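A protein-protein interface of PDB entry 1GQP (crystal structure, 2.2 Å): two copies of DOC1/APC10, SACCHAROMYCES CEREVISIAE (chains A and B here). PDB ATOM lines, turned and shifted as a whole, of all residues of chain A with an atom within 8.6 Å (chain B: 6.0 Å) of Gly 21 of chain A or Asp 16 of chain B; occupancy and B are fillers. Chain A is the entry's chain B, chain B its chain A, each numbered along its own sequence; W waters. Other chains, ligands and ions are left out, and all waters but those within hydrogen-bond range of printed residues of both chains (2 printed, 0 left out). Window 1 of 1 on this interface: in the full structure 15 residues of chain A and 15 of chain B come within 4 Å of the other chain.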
ATOM      1  N   ASP A   7      41.912  -0.007  18.456  1.00  0.00           N
ATOM      2  CA  ASP A   7      40.513   0.366  18.334  1.00  0.00           C
ATOM      3  C   ASP A   7      40.198   1.675  17.631  1.00  0.00           C
ATOM      4  O   ASP A   7      39.136   2.252  17.851  1.00  0.00           O
ATOM      5  CB  ASP A   7      39.848   0.357  19.713  1.00  0.00           C
ATOM      6  CG  ASP A   7      40.444   1.382  20.678  1.00  0.00           C
ATOM      7  OD1 ASP A   7      41.131   2.338  20.221  1.00  0.00           O
ATOM      8  OD2 ASP A   7      40.192   1.215  21.904  1.00  0.00           O
ATOM      9  N   LYS A  15      35.645  -6.134  14.626  1.00  0.00           N
ATOM     10  CA  LYS A  15      34.565  -5.381  15.265  1.00  0.00           C
ATOM     11  C   LYS A  15      34.091  -6.081  16.538  1.00  0.00           C
ATOM     12  O   LYS A  15      34.072  -5.489  17.625  1.00  0.00           O
ATOM     13  CB  LYS A  15      33.391  -5.219  14.291  1.00  0.00           C
ATOM     14  N   TYR A  18      36.235  -5.930  19.897  1.00  0.00           N
ATOM     15  CA  TYR A  18      36.113  -4.941  20.967  1.00  0.00           C
ATOM     16  C   TYR A  18      34.709  -4.946  21.584  1.00  0.00           C
ATOM     17  O   TYR A  18      33.736  -4.544  20.956  1.00  0.00           O
ATOM     18  CB  TYR A  18      36.466  -3.537  20.434  1.00  0.00           C
ATOM     19  CG  TYR A  18      37.776  -3.485  19.660  1.00  0.00           C
ATOM     20  CD1 TYR A  18      37.791  -3.605  18.273  1.00  0.00           C
ATOM     21  CD2 TYR A  18      39.004  -3.399  20.320  1.00  0.00           C
ATOM     22  CE1 TYR A  18      38.992  -3.648  17.558  1.00  0.00           C
ATOM     23  CE2 TYR A  18      40.222  -3.447  19.613  1.00  0.00           C
ATOM     24  CZ  TYR A  18      40.206  -3.575  18.232  1.00  0.00           C
ATOM     25  OH  TYR A  18      41.389  -3.669  17.513  1.00  0.00           O
ATOM     26  N   VAL A  19      34.604  -5.409  22.823  1.00  0.00           N
ATOM     27  CA  VAL A  19      33.310  -5.465  23.487  1.00  0.00           C
ATOM     28  C   VAL A  19      32.692  -4.077  23.645  1.00  0.00           C
ATOM     29  O   VAL A  19      31.468  -3.928  23.679  1.00  0.00           O
ATOM     30  CB  VAL A  19      33.437  -6.133  24.884  1.00  0.00           C
ATOM     31  CG1 VAL A  19      32.091  -6.105  25.618  1.00  0.00           C
ATOM     32  CG2 VAL A  19      33.930  -7.571  24.726  1.00  0.00           C
ATOM     33  N   ASN A  20      33.532  -3.056  23.747  1.00  0.00           N
ATOM     34  CA  ASN A  20      33.020  -1.702  23.913  1.00  0.00           C
ATOM     35  C   ASN A  20      32.980  -0.943  22.581  1.00  0.00           C
ATOM     36  O   ASN A  20      32.891  -1.547  21.505  1.00  0.00           O
ATOM     37  CB  ASN A  20      33.869  -0.957  24.954  1.00  0.00           C
ATOM     38  CG  ASN A  20      33.782  -1.592  26.337  1.00  0.00           C
ATOM     39  OD1 ASN A  20      34.721  -2.246  26.800  1.00  0.00           O
ATOM     40  ND2 ASN A  20      32.643  -1.412  26.999  1.00  0.00           N
ATOM     41  N   GLY A  21      33.035   0.377  22.642  1.00  0.00           N
ATOM     42  CA  GLY A  21      33.009   1.141  21.405  1.00  0.00           C
ATOM     43  C   GLY A  21      31.629   1.452  20.839  1.00  0.00           C
ATOM     44  O   GLY A  21      30.595   0.995  21.347  1.00  0.00           O
ATOM     45  N   PHE A  22      31.628   2.235  19.766  1.00  0.00           N
ATOM     46  CA  PHE A  22      30.402   2.647  19.106  1.00  0.00           C
ATOM     47  C   PHE A  22      30.530   2.593  17.571  1.00  0.00           C
ATOM     48  O   PHE A  22      31.325   3.330  16.978  1.00  0.00           O
ATOM     49  CB  PHE A  22      30.041   4.068  19.557  1.00  0.00           C
ATOM     50  CG  PHE A  22      28.771   4.587  18.957  1.00  0.00           C
ATOM     51  CD1 PHE A  22      27.538   4.099  19.380  1.00  0.00           C
ATOM     52  CD2 PHE A  22      28.809   5.531  17.930  1.00  0.00           C
ATOM     53  CE1 PHE A  22      26.357   4.545  18.787  1.00  0.00           C
ATOM     54  CE2 PHE A  22      27.636   5.985  17.326  1.00  0.00           C
ATOM     55  CZ  PHE A  22      26.408   5.493  17.750  1.00  0.00           C
ATOM     56  N   GLN A  23      29.752   1.720  16.937  1.00  0.00           N
ATOM     57  CA  GLN A  23      29.791   1.585  15.486  1.00  0.00           C
ATOM     58  C   GLN A  23      31.203   1.320  14.968  1.00  0.00           C
ATOM     59  O   GLN A  23      31.724   0.214  15.094  1.00  0.00           O
ATOM     60  CB  GLN A  23      29.252   2.853  14.827  1.00  0.00           C
ATOM     61  CG  GLN A  23      27.806   3.167  15.166  1.00  0.00           C
ATOM     62  CD  GLN A  23      27.322   4.474  14.540  1.00  0.00           C
ATOM     63  OE1 GLN A  23      26.165   4.859  14.705  1.00  0.00           O
ATOM     64  NE2 GLN A  23      28.211   5.161  13.823  1.00  0.00           N
ATOM     65  N   GLU A  25      34.196   0.867  17.160  1.00  0.00           N
ATOM     66  CA  GLU A  25      35.079   2.028  17.092  1.00  0.00           C
ATOM     67  C   GLU A  25      35.031   2.894  18.352  1.00  0.00           C
ATOM     68  O   GLU A  25      34.003   2.956  19.026  1.00  0.00           O
ATOM     69  CB  GLU A  25      34.740   2.851  15.854  1.00  0.00           C
ATOM     70  CG  GLU A  25      34.871   2.031  14.592  1.00  0.00           C
ATOM     71  CD  GLU A  25      35.167   2.873  13.374  1.00  0.00           C
ATOM     72  OE1 GLU A  25      34.248   3.562  12.886  1.00  0.00           O
ATOM     73  OE2 GLU A  25      36.327   2.851  12.906  1.00  0.00           O
ATOM     74  N   ILE A  26      36.155   3.548  18.660  1.00  0.00           N
ATOM     75  CA  ILE A  26      36.275   4.387  19.852  1.00  0.00           C
ATOM     76  C   ILE A  26      35.061   5.252  20.131  1.00  0.00           C
ATOM     77  O   ILE A  26      34.493   5.866  19.224  1.00  0.00           O
ATOM     78  CB  ILE A  26      37.491   5.351  19.791  1.00  0.00           C
ATOM     79  CG1 ILE A  26      37.408   6.210  18.529  1.00  0.00           C
ATOM     80  CG2 ILE A  26      38.798   4.577  19.858  1.00  0.00           C
ATOM     81  CD1 ILE A  26      38.397   7.367  18.518  1.00  0.00           C
ATOM     82  N   GLN A  27      34.681   5.298  21.405  1.00  0.00           N
ATOM     83  CA  GLN A  27      33.557   6.100  21.862  1.00  0.00           C
ATOM     84  C   GLN A  27      34.083   7.439  22.347  1.00  0.00           C
ATOM     85  O   GLN A  27      33.473   8.478  22.118  1.00  0.00           O
ATOM     86  CB  GLN A  27      32.829   5.403  23.017  1.00  0.00           C
ATOM     87  CG  GLN A  27      32.052   4.154  22.629  1.00  0.00           C
ATOM     88  CD  GLN A  27      31.611   3.351  23.843  1.00  0.00           C
ATOM     89  OE1 GLN A  27      30.500   3.518  24.360  1.00  0.00           O
ATOM     90  NE2 GLN A  27      32.496   2.483  24.315  1.00  0.00           N
ATOM     91  N   TYR A  28      35.226   7.398  23.021  1.00  0.00           N
ATOM     92  CA  TYR A  28      35.836   8.599  23.568  1.00  0.00           C
ATOM     93  C   TYR A  28      37.225   8.831  22.972  1.00  0.00           C
ATOM     94  O   TYR A  28      38.124   7.995  23.111  1.00  0.00           O
ATOM     95  CB  TYR A  28      35.948   8.469  25.090  1.00  0.00           C
ATOM     96  CG  TYR A  28      34.742   7.826  25.755  1.00  0.00           C
ATOM     97  CD1 TYR A  28      34.636   6.444  25.867  1.00  0.00           C
ATOM     98  CD2 TYR A  28      33.708   8.604  26.272  1.00  0.00           C
ATOM     99  CE1 TYR A  28      33.531   5.851  26.484  1.00  0.00           C
ATOM    100  CE2 TYR A  28      32.601   8.026  26.886  1.00  0.00           C
ATOM    101  CZ  TYR A  28      32.521   6.647  26.990  1.00  0.00           C
ATOM    102  OH  TYR A  28      31.438   6.076  27.612  1.00  0.00           O
ATOM    103  N   MET A  39      33.080   1.782  30.694  1.00  0.00           N
ATOM    104  CA  MET A  39      33.283   0.720  29.705  1.00  0.00           C
ATOM    105  C   MET A  39      33.612  -0.587  30.441  1.00  0.00           C
ATOM    106  O   MET A  39      33.091  -1.646  30.085  1.00  0.00           O
ATOM    107  CB  MET A  39      34.424   1.074  28.738  1.00  0.00           C
ATOM    108  CG  MET A  39      34.130   2.265  27.832  1.00  0.00           C
ATOM    109  SD  MET A  39      35.381   2.491  26.514  1.00  0.00           S
ATOM    110  CE  MET A  39      36.717   3.380  27.478  1.00  0.00           C
ATOM    111  N   GLN A  42      30.379  -1.851  31.863  1.00  0.00           N
ATOM    112  CA  GLN A  42      29.424  -2.182  30.787  1.00  0.00           C
ATOM    113  C   GLN A  42      29.852  -3.485  30.124  1.00  0.00           C
ATOM    114  O   GLN A  42      29.019  -4.331  29.815  1.00  0.00           O
ATOM    115  CB  GLN A  42      29.356  -1.062  29.731  1.00  0.00           C
ATOM    116  CG  GLN A  42      28.636   0.247  30.205  1.00  0.00           C
ATOM    117  CD  GLN A  42      27.095   0.100  30.306  1.00  0.00           C
ATOM    118  OE1 GLN A  42      26.475   0.441  31.323  1.00  0.00           O
ATOM    119  NE2 GLN A  42      26.488  -0.401  29.242  1.00  0.00           N
ATOM    120  N   GLY A  43      31.158  -3.629  29.906  1.00  0.00           N
ATOM    121  CA  GLY A  43      31.688  -4.832  29.289  1.00  0.00           C
ATOM    122  C   GLY A  43      31.329  -6.091  30.060  1.00  0.00           C
ATOM    123  O   GLY A  43      30.984  -7.113  29.466  1.00  0.00           O
ATOM    124  N   ILE A  46      27.644  -6.904  29.471  1.00  0.00           N
ATOM    125  CA  ILE A  46      27.434  -7.448  28.146  1.00  0.00           C
ATOM    126  C   ILE A  46      27.895  -8.905  28.026  1.00  0.00           C
ATOM    127  O   ILE A  46      27.176  -9.737  27.466  1.00  0.00           O
ATOM    128  CB  ILE A  46      28.129  -6.565  27.117  1.00  0.00           C
ATOM    129  CG1 ILE A  46      27.397  -5.213  27.069  1.00  0.00           C
ATOM    130  CG2 ILE A  46      28.172  -7.267  25.741  1.00  0.00           C
ATOM    131  CD1 ILE A  46      28.080  -4.174  26.199  1.00  0.00           C
ATOM    132  N   ASN A 147      41.477   0.668  24.832  1.00  0.00           N
ATOM    133  CA  ASN A 147      40.935   1.127  26.109  1.00  0.00           C
ATOM    134  C   ASN A 147      39.550   0.488  26.192  1.00  0.00           C
ATOM    135  O   ASN A 147      38.597   1.010  25.636  1.00  0.00           O
ATOM    136  CB  ASN A 147      40.838   2.667  26.158  1.00  0.00           C
ATOM    137  CG  ASN A 147      42.205   3.349  26.268  1.00  0.00           C
ATOM    138  OD1 ASN A 147      42.818   3.403  27.345  1.00  0.00           O
ATOM    139  ND2 ASN A 147      42.692   3.859  25.144  1.00  0.00           N
ATOM    140  N   GLY A 148      39.470  -0.659  26.866  1.00  0.00           N
ATOM    141  CA  GLY A 148      38.225  -1.378  27.011  1.00  0.00           C
ATOM    142  C   GLY A 148      38.402  -2.901  26.997  1.00  0.00           C
ATOM    143  O   GLY A 148      39.529  -3.417  27.015  1.00  0.00           O
ATOM    144  N   TRP A 149      37.284  -3.622  26.989  1.00  0.00           N
ATOM    145  CA  TRP A 149      37.306  -5.080  26.943  1.00  0.00           C
ATOM    146  C   TRP A 149      37.482  -5.641  25.531  1.00  0.00           C
ATOM    147  O   TRP A 149      36.842  -5.172  24.582  1.00  0.00           O
ATOM    148  CB  TRP A 149      36.005  -5.651  27.492  1.00  0.00           C
ATOM    149  CG  TRP A 149      35.906  -5.633  28.982  1.00  0.00           C
ATOM    150  CD1 TRP A 149      35.202  -4.745  29.744  1.00  0.00           C
ATOM    151  CD2 TRP A 149      36.456  -6.597  29.887  1.00  0.00           C
ATOM    152  NE1 TRP A 149      35.265  -5.108  31.069  1.00  0.00           N
ATOM    153  CE2 TRP A 149      36.027  -6.243  31.187  1.00  0.00           C
ATOM    154  CE3 TRP A 149      37.262  -7.736  29.725  1.00  0.00           C
ATOM    155  CZ2 TRP A 149      36.386  -6.981  32.332  1.00  0.00           C
ATOM    156  CZ3 TRP A 149      37.620  -8.474  30.861  1.00  0.00           C
ATOM    157  CH2 TRP A 149      37.175  -8.092  32.147  1.00  0.00           C
ATOM    158  N   ALA B  12      23.977  -7.473  23.860  1.00  0.00           N
ATOM    159  CA  ALA B  12      25.037  -7.103  22.938  1.00  0.00           C
ATOM    160  C   ALA B  12      24.442  -6.562  21.648  1.00  0.00           C
ATOM    161  O   ALA B  12      25.018  -5.688  20.995  1.00  0.00           O
ATOM    162  CB  ALA B  12      25.922  -8.338  22.630  1.00  0.00           C
ATOM    163  N   ALA B  13      23.284  -7.100  21.284  1.00  0.00           N
ATOM    164  CA  ALA B  13      22.591  -6.715  20.058  1.00  0.00           C
ATOM    165  C   ALA B  13      22.096  -5.269  20.067  1.00  0.00           C
ATOM    166  O   ALA B  13      21.941  -4.659  19.019  1.00  0.00           O
ATOM    167  CB  ALA B  13      21.402  -7.671  19.825  1.00  0.00           C
ATOM    168  N   THR B  14      21.858  -4.714  21.245  1.00  0.00           N
ATOM    169  CA  THR B  14      21.351  -3.352  21.316  1.00  0.00           C
ATOM    170  C   THR B  14      22.323  -2.359  21.924  1.00  0.00           C
ATOM    171  O   THR B  14      21.938  -1.237  22.279  1.00  0.00           O
ATOM    172  CB  THR B  14      20.076  -3.314  22.132  1.00  0.00           C
ATOM    173  OG1 THR B  14      20.330  -3.858  23.431  1.00  0.00           O
ATOM    174  CG2 THR B  14      18.996  -4.138  21.447  1.00  0.00           C
ATOM    175  N   LYS B  15      23.586  -2.745  22.047  1.00  0.00           N
ATOM    176  CA  LYS B  15      24.534  -1.835  22.672  1.00  0.00           C
ATOM    177  C   LYS B  15      24.677  -0.505  21.919  1.00  0.00           C
ATOM    178  O   LYS B  15      24.839   0.535  22.549  1.00  0.00           O
ATOM    179  CB  LYS B  15      25.910  -2.502  22.847  1.00  0.00           C
ATOM    180  CG  LYS B  15      26.733  -2.600  21.581  1.00  0.00           C
ATOM    181  CD  LYS B  15      28.239  -2.464  21.871  1.00  0.00           C
ATOM    182  CE  LYS B  15      29.050  -2.497  20.570  1.00  0.00           C
ATOM    183  NZ  LYS B  15      30.380  -1.806  20.648  1.00  0.00           N
ATOM    184  N   ASP B  16      24.618  -0.521  20.591  1.00  0.00           N
ATOM    185  CA  ASP B  16      24.760   0.736  19.864  1.00  0.00           C
ATOM    186  C   ASP B  16      23.446   1.542  19.807  1.00  0.00           C
ATOM    187  O   ASP B  16      23.417   2.675  19.320  1.00  0.00           O
ATOM    188  CB  ASP B  16      25.320   0.508  18.443  1.00  0.00           C
ATOM    189  CG  ASP B  16      26.790   0.036  18.445  1.00  0.00           C
ATOM    190  OD1 ASP B  16      27.551   0.391  19.379  1.00  0.00           O
ATOM    191  OD2 ASP B  16      27.191  -0.676  17.500  1.00  0.00           O
ATOM    192  N   LEU B  17      22.357   0.964  20.300  1.00  0.00           N
ATOM    193  CA  LEU B  17      21.082   1.671  20.323  1.00  0.00           C
ATOM    194  C   LEU B  17      21.148   2.605  21.530  1.00  0.00           C
ATOM    195  O   LEU B  17      20.797   3.780  21.442  1.00  0.00           O
ATOM    196  CB  LEU B  17      19.924   0.681  20.492  1.00  0.00           C
ATOM    197  CG  LEU B  17      18.517   1.256  20.711  1.00  0.00           C
ATOM    198  CD1 LEU B  17      18.062   2.065  19.476  1.00  0.00           C
ATOM    199  CD2 LEU B  17      17.560   0.099  20.997  1.00  0.00           C
ATOM    200  N   TYR B  18      21.632   2.071  22.649  1.00  0.00           N
ATOM    201  CA  TYR B  18      21.753   2.823  23.875  1.00  0.00           C
ATOM    202  C   TYR B  18      23.143   3.439  23.991  1.00  0.00           C
ATOM    203  O   TYR B  18      24.081   2.828  24.526  1.00  0.00           O
ATOM    204  CB  TYR B  18      21.438   1.898  25.062  1.00  0.00           C
ATOM    205  CG  TYR B  18      20.063   1.256  24.936  1.00  0.00           C
ATOM    206  CD1 TYR B  18      19.911  -0.103  24.618  1.00  0.00           C
ATOM    207  CD2 TYR B  18      18.907   2.021  25.093  1.00  0.00           C
ATOM    208  CE1 TYR B  18      18.622  -0.675  24.463  1.00  0.00           C
ATOM    209  CE2 TYR B  18      17.638   1.459  24.937  1.00  0.00           C
ATOM    210  CZ  TYR B  18      17.500   0.127  24.626  1.00  0.00           C
ATOM    211  OH  TYR B  18      16.230  -0.373  24.471  1.00  0.00           O
ATOM    212  N   VAL B  19      23.248   4.662  23.484  1.00  0.00           N
ATOM    213  CA  VAL B  19      24.490   5.413  23.454  1.00  0.00           C
ATOM    214  C   VAL B  19      25.159   5.574  24.797  1.00  0.00           C
ATOM    215  O   VAL B  19      26.386   5.579  24.895  1.00  0.00           O
ATOM    216  CB  VAL B  19      24.268   6.824  22.869  1.00  0.00           C
ATOM    217  CG1 VAL B  19      25.585   7.615  22.930  1.00  0.00           C
ATOM    218  CG2 VAL B  19      23.763   6.723  21.424  1.00  0.00           C
ATOM    219  N   VAL B 150      19.344   7.740  22.472  1.00  0.00           N
ATOM    220  CA  VAL B 150      18.987   6.571  21.696  1.00  0.00           C
ATOM    221  C   VAL B 150      19.358   6.892  20.252  1.00  0.00           C
ATOM    222  O   VAL B 150      19.022   7.958  19.718  1.00  0.00           O
ATOM    223  CB  VAL B 150      17.476   6.254  21.837  1.00  0.00           C
ATOM    224  CG1 VAL B 150      17.083   5.127  20.902  1.00  0.00           C
ATOM    225  CG2 VAL B 150      17.178   5.845  23.273  1.00  0.00           C
ATOM    226  N   ALA B 151      20.085   5.971  19.633  1.00  0.00           N
ATOM    227  CA  ALA B 151      20.536   6.132  18.255  1.00  0.00           C
ATOM    228  C   ALA B 151      19.782   5.136  17.375  1.00  0.00           C
ATOM    229  O   ALA B 151      20.043   3.925  17.400  1.00  0.00           O
ATOM    230  CB  ALA B 151      22.029   5.875  18.173  1.00  0.00           C
ATOM    231  N   ARG B 153      18.837   3.477  13.923  1.00  0.00           N
ATOM    232  CA  ARG B 153      19.442   3.171  12.628  1.00  0.00           C
ATOM    233  C   ARG B 153      18.364   2.856  11.591  1.00  0.00           C
ATOM    234  O   ARG B 153      18.668   2.480  10.460  1.00  0.00           O
ATOM    235  CB  ARG B 153      20.367   1.956  12.737  1.00  0.00           C
ATOM    236  CG  ARG B 153      21.409   2.001  13.839  1.00  0.00           C
ATOM    237  CD  ARG B 153      22.393   3.121  13.630  1.00  0.00           C
ATOM    238  NE  ARG B 153      23.600   2.987  14.455  1.00  0.00           N
ATOM    239  CZ  ARG B 153      23.611   2.854  15.781  1.00  0.00           C
ATOM    240  NH1 ARG B 153      22.482   2.822  16.465  1.00  0.00           N
ATOM    241  NH2 ARG B 153      24.765   2.780  16.430  1.00  0.00           N
HETATM  242  O   HOH W   1      30.089  -1.226  17.759  1.00  0.00           O
HETATM  243  O   HOH W   2      28.169   4.178  23.293  1.00  0.00           O
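The backbone NH of Gly 21 of chain A sits close to the side-chain amide nitrogen of Gln 27 of chain A (2.7 Å). NH1 of Arg 153 of chain B is in hydrogen-bond range of O of Ala 151 of chain B (2.8 Å). The side-chain amide oxygen (OD1) of Asn 20 of chain A sits at hydrogen-bond distance from the backbone NH (N) of Trp 149 of chain A (2.9 Å). The guanidinium group (NH1) of Arg 153 of chain B sits at hydrogen-bond distance from the backbone carbonyl oxygen (O) of Asp 16 of chain B, at 3.0 Å. O of Trp 149 of chain A lies within hydrogen-bond range of N of Val 19 of chain A (2.9 Å). The side-chain amino group (NZ) of Lys 15 of chain B is in salt-bridge range of the side-chain carboxylate (OD1) of Asp 16 of chain B.
Printed residues of chain B within 4 Å of Asn 20 of chain A: Lys 15 (2.7 Å). Gly 21 of chain A touches just these residues of chain B: Lys 15 (2.9 Å) and Asp 16 (3.7 Å). Of the printed residues of chain B, Phe 22 of chain A touches Asp 16 and Arg 153. Gln 27 of chain A touches none of the printed residues of chain B. Printed residues of chain B within 4 Å of Ile 46 of chain A: Ala 12 (3.99 Å). Printed residues of chain A within 4 Å of Ala 12 of chain B: Ile 46 (3.99 Å). Of chain A, only Val 19, Asn 20 and Gly 21 come within 4 Å of Lys 15 of chain B. Val 150 of chain B touches none of the printed residues of chain A. Of the printed residues of chain A, Arg 153 of chain B touches Phe 22 and Gln 23. The nearest printed residue of chain B that does not touch Val 19 of chain A is Ala 12 of chain B (7.2 Å).
NZ of Lys 15 of chain B sits at hydrogen-bond distance from O of Asn 20 of chain A, 2.7 Å away. O of Gly 21 of chain A lies within hydrogen-bond range of NZ of Lys 15 of chain B, at 2.9 Å. OE1 of Gln 23 of chain A is in hydrogen-bond range of NH2 of Arg 153 of chain B.
Val 19 of chain A touches Lys 15 of chain B, but with the chains exchanged Lys 15 of chain A does not touch Val 19 of chain B (15.3 Å).
NZ of Lys 15 of chain B touches O of Val 19 of chain A (3.9 Å). Gly 21 of chain A touches Asp 16 of chain B. Phe 22 of chain A touches Asp 16 of chain B (CE1 to O, 3.5 Å). Phe 22 of chain A touches Arg 153 of chain B (CE1 to NH2, 3.3 Å). Gln 23 of chain A touches Asp 16 of chain B. Ile 46 of chain A touches Ala 12 of chain B (CG2 to CB, 3.99 Å).
Hydrophobic or aromatic side chains of chain A that line the printed part of chain B: Phe 22 and Ile 46. Of the 11 printed residues of chain B, 4 touch a printed residue of chain A. Among the printed residues, no Asp or Glu carboxylate lies within 4 Å of a Lys or Arg side-chain nitrogen of the other chain.
Water W2 lies within hydrogen-bond range of OE1 of Gln 27 of chain A (2.6 Å) and O of Val 19 of chain B (2.8 Å). Water W1 lies within hydrogen-bond range of the side-chain amino group (NZ) of Lys 15 of chain B (3.0 Å), the side-chain carboxylate (OD2) of Asp 16 of chain B (3.0 Å) and the backbone NH (N) of Gln 23 of chain A (3.1 Å).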
